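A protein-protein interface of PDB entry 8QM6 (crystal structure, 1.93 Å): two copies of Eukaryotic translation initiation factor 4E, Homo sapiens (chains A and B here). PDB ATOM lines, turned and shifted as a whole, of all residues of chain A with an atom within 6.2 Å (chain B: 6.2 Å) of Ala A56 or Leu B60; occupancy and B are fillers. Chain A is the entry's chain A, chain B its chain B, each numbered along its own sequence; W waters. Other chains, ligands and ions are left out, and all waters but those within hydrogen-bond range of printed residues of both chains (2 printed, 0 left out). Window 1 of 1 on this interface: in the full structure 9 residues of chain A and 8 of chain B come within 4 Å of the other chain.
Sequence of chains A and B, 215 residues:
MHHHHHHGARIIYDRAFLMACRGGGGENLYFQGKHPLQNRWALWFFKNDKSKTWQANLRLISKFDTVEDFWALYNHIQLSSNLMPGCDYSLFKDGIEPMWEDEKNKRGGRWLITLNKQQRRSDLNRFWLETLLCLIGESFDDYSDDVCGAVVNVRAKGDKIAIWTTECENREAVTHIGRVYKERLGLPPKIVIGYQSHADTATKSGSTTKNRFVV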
ATOM      1  N   LYS A  52      11.967  -5.773   0.690  1.00  0.00           N
ATOM      2  CA  LYS A  52      12.700  -5.272  -0.459  1.00  0.00           C
ATOM      3  C   LYS A  52      11.792  -4.406  -1.331  1.00  0.00           C
ATOM      4  O   LYS A  52      10.567  -4.549  -1.290  1.00  0.00           O
ATOM      5  CB  LYS A  52      13.269  -6.454  -1.264  1.00  0.00           C
ATOM      6  CG  LYS A  52      14.007  -7.520  -0.437  1.00  0.00           C
ATOM      7  CD  LYS A  52      14.507  -8.643  -1.345  1.00  0.00           C
ATOM      8  CE  LYS A  52      15.460  -9.592  -0.674  1.00  0.00           C
ATOM      9  NZ  LYS A  52      14.816 -10.907  -0.355  1.00  0.00           N
ATOM     10  N   THR A  53      12.387  -3.498  -2.122  1.00  0.00           N
ATOM     11  CA  THR A  53      11.619  -2.716  -3.094  1.00  0.00           C
ATOM     12  C   THR A  53      11.074  -3.651  -4.196  1.00  0.00           C
ATOM     13  O   THR A  53      11.647  -4.726  -4.422  1.00  0.00           O
ATOM     14  CB  THR A  53      12.496  -1.612  -3.759  1.00  0.00           C
ATOM     15  OG1 THR A  53      13.486  -2.229  -4.593  1.00  0.00           O
ATOM     16  CG2 THR A  53      13.159  -0.683  -2.743  1.00  0.00           C
ATOM     17  N   TRP A  54       9.987  -3.255  -4.897  1.00  0.00           N
ATOM     18  CA  TRP A  54       9.460  -4.064  -6.006  1.00  0.00           C
ATOM     19  C   TRP A  54      10.511  -4.357  -7.071  1.00  0.00           C
ATOM     20  O   TRP A  54      10.442  -5.397  -7.717  1.00  0.00           O
ATOM     21  CB  TRP A  54       8.196  -3.430  -6.673  1.00  0.00           C
ATOM     22  CG  TRP A  54       8.399  -2.075  -7.296  1.00  0.00           C
ATOM     23  CD1 TRP A  54       8.146  -0.865  -6.716  1.00  0.00           C
ATOM     24  CD2 TRP A  54       8.866  -1.791  -8.631  1.00  0.00           C
ATOM     25  NE1 TRP A  54       8.446   0.154  -7.597  1.00  0.00           N
ATOM     26  CE2 TRP A  54       8.893  -0.386  -8.776  1.00  0.00           C
ATOM     27  CE3 TRP A  54       9.277  -2.586  -9.709  1.00  0.00           C
ATOM     28  CZ2 TRP A  54       9.308   0.237  -9.960  1.00  0.00           C
ATOM     29  CZ3 TRP A  54       9.696  -1.971 -10.876  1.00  0.00           C
ATOM     30  CH2 TRP A  54       9.702  -0.574 -10.998  1.00  0.00           C
ATOM     31  N   GLN A  55      11.481  -3.454  -7.253  1.00  0.00           N
ATOM     32  CA  GLN A  55      12.516  -3.635  -8.259  1.00  0.00           C
ATOM     33  C   GLN A  55      13.383  -4.862  -7.879  1.00  0.00           C
ATOM     34  O   GLN A  55      13.672  -5.715  -8.714  1.00  0.00           O
ATOM     35  CB  GLN A  55      13.373  -2.356  -8.359  1.00  0.00           C
ATOM     36  CG  GLN A  55      12.579  -1.081  -8.638  1.00  0.00           C
ATOM     37  CD  GLN A  55      12.305  -0.341  -7.356  1.00  0.00           C
ATOM     38  OE1 GLN A  55      11.290  -0.601  -6.682  1.00  0.00           O
ATOM     39  NE2 GLN A  55      13.210   0.587  -6.991  1.00  0.00           N
ATOM     40  N   ALA A  56      13.764  -4.943  -6.626  1.00  0.00           N
ATOM     41  CA  ALA A  56      14.632  -5.998  -6.133  1.00  0.00           C
ATOM     42  C   ALA A  56      13.978  -7.381  -6.208  1.00  0.00           C
ATOM     43  O   ALA A  56      14.678  -8.364  -6.380  1.00  0.00           O
ATOM     44  CB  ALA A  56      15.051  -5.685  -4.703  1.00  0.00           C
ATOM     45  N   ASN A  57      12.653  -7.478  -6.130  1.00  0.00           N
ATOM     46  CA  ASN A  57      11.982  -8.780  -6.154  1.00  0.00           C
ATOM     47  C   ASN A  57      11.678  -9.313  -7.578  1.00  0.00           C
ATOM     48  O   ASN A  57      11.416 -10.510  -7.726  1.00  0.00           O
ATOM     49  CB  ASN A  57      10.723  -8.694  -5.342  1.00  0.00           C
ATOM     50  CG  ASN A  57      10.978  -8.600  -3.847  1.00  0.00           C
ATOM     51  OD1 ASN A  57      11.859  -9.270  -3.273  1.00  0.00           O
ATOM     52  ND2 ASN A  57      10.204  -7.789  -3.188  1.00  0.00           N
ATOM     53  N   LEU A  58      11.715  -8.445  -8.588  1.00  0.00           N
ATOM     54  CA  LEU A  58      11.498  -8.800  -9.982  1.00  0.00           C
ATOM     55  C   LEU A  58      12.793  -9.203 -10.637  1.00  0.00           C
ATOM     56  O   LEU A  58      13.719  -8.378 -10.748  1.00  0.00           O
ATOM     57  CB  LEU A  58      10.867  -7.599 -10.730  1.00  0.00           C
ATOM     58  CG  LEU A  58      10.548  -7.831 -12.189  1.00  0.00           C
ATOM     59  CD1 LEU A  58       9.450  -8.941 -12.370  1.00  0.00           C
ATOM     60  CD2 LEU A  58      10.204  -6.542 -12.880  1.00  0.00           C
ATOM     61  N   ARG A  59      12.875 -10.460 -11.080  1.00  0.00           N
ATOM     62  CA  ARG A  59      14.043 -11.023 -11.749  1.00  0.00           C
ATOM     63  C   ARG A  59      13.718 -11.484 -13.160  1.00  0.00           C
ATOM     64  O   ARG A  59      12.708 -12.160 -13.364  1.00  0.00           O
ATOM     65  CB  ARG A  59      14.564 -12.249 -10.927  1.00  0.00           C
ATOM     66  CG  ARG A  59      15.660 -11.923  -9.908  1.00  0.00           C
ATOM     67  CD  ARG A  59      16.909 -12.761 -10.142  1.00  0.00           C
ATOM     68  NE  ARG A  59      17.383 -12.639 -11.523  1.00  0.00           N
ATOM     69  CZ  ARG A  59      18.204 -13.491 -12.135  1.00  0.00           C
ATOM     70  NH1 ARG A  59      18.569 -13.278 -13.399  1.00  0.00           N
ATOM     71  NH2 ARG A  59      18.673 -14.555 -11.490  1.00  0.00           N
ATOM     72  N   ALA B  42      21.274  -4.067 -12.755  1.00  0.00           N
ATOM     73  CA  ALA B  42      20.768  -3.342 -11.593  1.00  0.00           C
ATOM     74  C   ALA B  42      21.829  -2.348 -11.067  1.00  0.00           C
ATOM     75  O   ALA B  42      23.008  -2.717 -10.846  1.00  0.00           O
ATOM     76  CB  ALA B  42      20.398  -4.330 -10.499  1.00  0.00           C
ATOM     77  N   LEU B  43      21.403  -1.106 -10.879  1.00  0.00           N
ATOM     78  CA  LEU B  43      22.212  -0.023 -10.342  1.00  0.00           C
ATOM     79  C   LEU B  43      21.956   0.100  -8.876  1.00  0.00           C
ATOM     80  O   LEU B  43      20.794   0.265  -8.458  1.00  0.00           O
ATOM     81  CB  LEU B  43      21.884   1.327 -11.004  1.00  0.00           C
ATOM     82  CG  LEU B  43      22.642   2.548 -10.461  1.00  0.00           C
ATOM     83  CD1 LEU B  43      24.156   2.360 -10.604  1.00  0.00           C
ATOM     84  CD2 LEU B  43      22.156   3.788 -11.119  1.00  0.00           C
ATOM     85  N   TRP B  44      23.036   0.040  -8.114  1.00  0.00           N
ATOM     86  CA  TRP B  44      23.057   0.104  -6.696  1.00  0.00           C
ATOM     87  C   TRP B  44      23.862   1.299  -6.233  1.00  0.00           C
ATOM     88  O   TRP B  44      24.804   1.750  -6.901  1.00  0.00           O
ATOM     89  CB  TRP B  44      23.748  -1.130  -6.100  1.00  0.00           C
ATOM     90  CG  TRP B  44      23.180  -2.434  -6.510  1.00  0.00           C
ATOM     91  CD1 TRP B  44      23.401  -3.114  -7.668  1.00  0.00           C
ATOM     92  CD2 TRP B  44      22.286  -3.228  -5.735  1.00  0.00           C
ATOM     93  NE1 TRP B  44      22.674  -4.285  -7.671  1.00  0.00           N
ATOM     94  CE2 TRP B  44      22.012  -4.399  -6.479  1.00  0.00           C
ATOM     95  CE3 TRP B  44      21.741  -3.097  -4.458  1.00  0.00           C
ATOM     96  CZ2 TRP B  44      21.199  -5.414  -5.994  1.00  0.00           C
ATOM     97  CZ3 TRP B  44      20.905  -4.103  -3.980  1.00  0.00           C
ATOM     98  CH2 TRP B  44      20.641  -5.240  -4.743  1.00  0.00           C
ATOM     99  N   PHE B  45      23.495   1.772  -5.047  1.00  0.00           N
ATOM    100  CA  PHE B  45      24.148   2.852  -4.332  1.00  0.00           C
ATOM    101  C   PHE B  45      24.446   2.396  -2.920  1.00  0.00           C
ATOM    102  O   PHE B  45      23.610   1.746  -2.297  1.00  0.00           O
ATOM    103  CB  PHE B  45      23.228   4.075  -4.329  1.00  0.00           C
ATOM    104  CG  PHE B  45      23.775   5.258  -3.591  1.00  0.00           C
ATOM    105  CD1 PHE B  45      24.789   6.022  -4.133  1.00  0.00           C
ATOM    106  CD2 PHE B  45      23.253   5.632  -2.367  1.00  0.00           C
ATOM    107  CE1 PHE B  45      25.282   7.134  -3.461  1.00  0.00           C
ATOM    108  CE2 PHE B  45      23.765   6.727  -1.680  1.00  0.00           C
ATOM    109  CZ  PHE B  45      24.782   7.467  -2.230  1.00  0.00           C
ATOM    110  N   LEU B  58      22.646  -0.167   1.715  1.00  0.00           N
ATOM    111  CA  LEU B  58      22.619  -0.638   0.334  1.00  0.00           C
ATOM    112  C   LEU B  58      21.270  -0.404  -0.324  1.00  0.00           C
ATOM    113  O   LEU B  58      20.265  -1.016   0.058  1.00  0.00           O
ATOM    114  CB  LEU B  58      22.970  -2.121   0.288  1.00  0.00           C
ATOM    115  CG  LEU B  58      23.112  -2.735  -1.109  1.00  0.00           C
ATOM    116  CD1 LEU B  58      24.177  -1.989  -1.983  1.00  0.00           C
ATOM    117  CD2 LEU B  58      23.376  -4.249  -1.029  1.00  0.00           C
ATOM    118  N   ARG B  59      21.234   0.469  -1.322  1.00  0.00           N
ATOM    119  CA  ARG B  59      20.000   0.814  -2.007  1.00  0.00           C
ATOM    120  C   ARG B  59      20.066   0.349  -3.448  1.00  0.00           C
ATOM    121  O   ARG B  59      21.019   0.673  -4.144  1.00  0.00           O
ATOM    122  CB  ARG B  59      19.793   2.338  -1.964  1.00  0.00           C
ATOM    123  CG  ARG B  59      18.579   2.828  -1.184  1.00  0.00           C
ATOM    124  CD  ARG B  59      18.781   4.255  -0.696  1.00  0.00           C
ATOM    125  NE  ARG B  59      19.536   4.306   0.562  1.00  0.00           N
ATOM    126  CZ  ARG B  59      19.028   4.066   1.772  1.00  0.00           C
ATOM    127  NH1 ARG B  59      19.803   4.140   2.851  1.00  0.00           N
ATOM    128  NH2 ARG B  59      17.741   3.749   1.915  1.00  0.00           N
ATOM    129  N   LEU B  60      19.072  -0.416  -3.886  1.00  0.00           N
ATOM    130  CA  LEU B  60      18.821  -0.623  -5.304  1.00  0.00           C
ATOM    131  C   LEU B  60      18.146   0.610  -5.868  1.00  0.00           C
ATOM    132  O   LEU B  60      17.079   0.990  -5.401  1.00  0.00           O
ATOM    133  CB  LEU B  60      17.914  -1.815  -5.511  1.00  0.00           C
ATOM    134  CG  LEU B  60      17.483  -2.097  -6.934  1.00  0.00           C
ATOM    135  CD1 LEU B  60      18.628  -2.528  -7.783  1.00  0.00           C
ATOM    136  CD2 LEU B  60      16.460  -3.139  -6.948  1.00  0.00           C
ATOM    137  N   ILE B  61      18.737   1.224  -6.881  1.00  0.00           N
ATOM    138  CA  ILE B  61      18.151   2.415  -7.516  1.00  0.00           C
ATOM    139  C   ILE B  61      17.193   2.000  -8.603  1.00  0.00           C
ATOM    140  O   ILE B  61      16.051   2.468  -8.638  1.00  0.00           O
ATOM    141  CB  ILE B  61      19.282   3.353  -8.060  1.00  0.00           C
ATOM    142  CG1 ILE B  61      20.240   3.815  -6.937  1.00  0.00           C
ATOM    143  CG2 ILE B  61      18.715   4.523  -8.860  1.00  0.00           C
ATOM    144  CD1 ILE B  61      19.599   4.315  -5.665  1.00  0.00           C
ATOM    145  N   SER B  62      17.629   1.126  -9.509  1.00  0.00           N
ATOM    146  CA  SER B  62      16.869   0.862 -10.725  1.00  0.00           C
ATOM    147  C   SER B  62      17.434  -0.331 -11.472  1.00  0.00           C
ATOM    148  O   SER B  62      18.592  -0.690 -11.245  1.00  0.00           O
ATOM    149  CB  SER B  62      16.850   2.118 -11.611  1.00  0.00           C
ATOM    150  OG  SER B  62      15.873   1.942 -12.628  1.00  0.00           O
ATOM    151  N   LYS B  63      16.629  -0.937 -12.348  1.00  0.00           N
ATOM    152  CA  LYS B  63      17.043  -1.990 -13.274  1.00  0.00           C
ATOM    153  C   LYS B  63      16.589  -1.679 -14.652  1.00  0.00           C
ATOM    154  O   LYS B  63      15.606  -0.963 -14.833  1.00  0.00           O
ATOM    155  CB  LYS B  63      16.494  -3.353 -12.892  1.00  0.00           C
ATOM    156  CG  LYS B  63      16.744  -3.729 -11.453  1.00  0.00           C
ATOM    157  CD  LYS B  63      16.423  -5.191 -11.212  1.00  0.00           C
ATOM    158  CE  LYS B  63      16.651  -5.637  -9.814  1.00  0.00           C
ATOM    159  NZ  LYS B  63      16.293  -7.081  -9.657  1.00  0.00           N
ATOM    160  N   ASP B  94      21.480  -8.656 -13.079  1.00  0.00           N
ATOM    161  CA  ASP B  94      20.290  -8.927 -12.278  1.00  0.00           C
ATOM    162  C   ASP B  94      20.442 -10.249 -11.497  1.00  0.00           C
ATOM    163  O   ASP B  94      20.737 -11.265 -12.116  1.00  0.00           O
ATOM    164  CB  ASP B  94      19.101  -8.961 -13.229  1.00  0.00           C
ATOM    165  CG  ASP B  94      17.725  -9.033 -12.597  1.00  0.00           C
ATOM    166  OD1 ASP B  94      17.579  -8.636 -11.415  1.00  0.00           O
ATOM    167  OD2 ASP B  94      16.818  -9.453 -13.271  1.00  0.00           O
HETATM  168  O   HOH W   1      21.318 -11.972 -14.602  1.00  0.00           O
HETATM  169  O   HOH W   2      17.545  -7.718  -7.059  1.00  0.00           O
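Water W1 bridges the backbone carbonyl oxygen of Asp B94 (2.6 Å) and the guanidinium group of Arg A59 (3.3 Å).
Water W2 lies within hydrogen-bond range of the side-chain amino group (NZ) of Lys B63 (3.0 Å) and the backbone carbonyl oxygen (O) of Ala A56 (3.0 Å).
Among the printed residues, pairs that only touch across the chains: Ala A56 with Leu B60 (3.3 Å), Gln A55 with Leu B60 (3.5 Å), Gln A55 with Ile B61 (3.8 Å), Ala A56 with Lys B63 (3.9 Å), Thr A53 with Leu B60 (3.9 Å) and Leu A58 with Asp B94 (3.9 Å).
Hydrophobic or aromatic side chains of chain A within 4 Å of the printed part of chain B: Ala A56.
Among the printed residues, 9 pairs touch across the chains.
Among the printed residues, Asp or Glu carboxylates within 4 Å of a Lys or Arg side-chain nitrogen of the other chain: Arg A59 with Asp B94.
O of Gln A55 is in hydrogen-bond range of NZ of Lys B63 (3.1 Å).
The side-chain amino group (NZ) of Lys B63 is in hydrogen-bond range of the backbone carbonyl oxygen (O) of Leu A58 (3.1 Å).
The side-chain carboxylate (OD2) of Asp B94 is in salt-bridge range of the guanidinium group (NE) of Arg A59.
OE1 of Gln A55 lies close to OG1 of Thr A53.
The side-chain hydroxyl (OG1) of Thr A53 sits at hydrogen-bond distance from the backbone NH (N) of Ala A56, at 3.4 Å.
The indole nitrogen (NE1) of Trp A54 is in hydrogen-bond range of the side-chain amide oxygen (OE1) of Gln A55 (3.1 Å).
The backbone carbonyl oxygen (O) of Leu B43 is in hydrogen-bond range of the backbone NH (N) of Ile B61.
The side-chain amino group of Lys B63 lies within salt-bridge range of the side-chain carboxylate of Asp B94 (2.7 Å).
2 positions are printed for both chains.
Of the 9 pairs that touch across the chains among the printed residues, none has its exchanged pair printed and touching as well.
Of chain B, only Leu B60 and Lys B63 come within 4 Å of Ala A56.
Of the printed residues of chain A, Leu B60 touches Thr A53 (3.9 Å), Gln A55 (3.5 Å) and Ala A56 (3.3 Å).
Printed residues of chain A within 4 Å of Asp B94: Leu A58 and Arg A59.
Of the printed residues of chain B, Thr A53 touches Leu B60.
Printed residues of chain B within 4 Å of Arg A59: Asp B94.
Asn A57 touches none of the printed residues of chain B.
The nearest residue of chain B that does not touch Ala A56 is Trp B44 (5.6 Å).
The nearest printed residue of chain A that does not touch Lys B63 is Arg A59 (4.9 Å).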
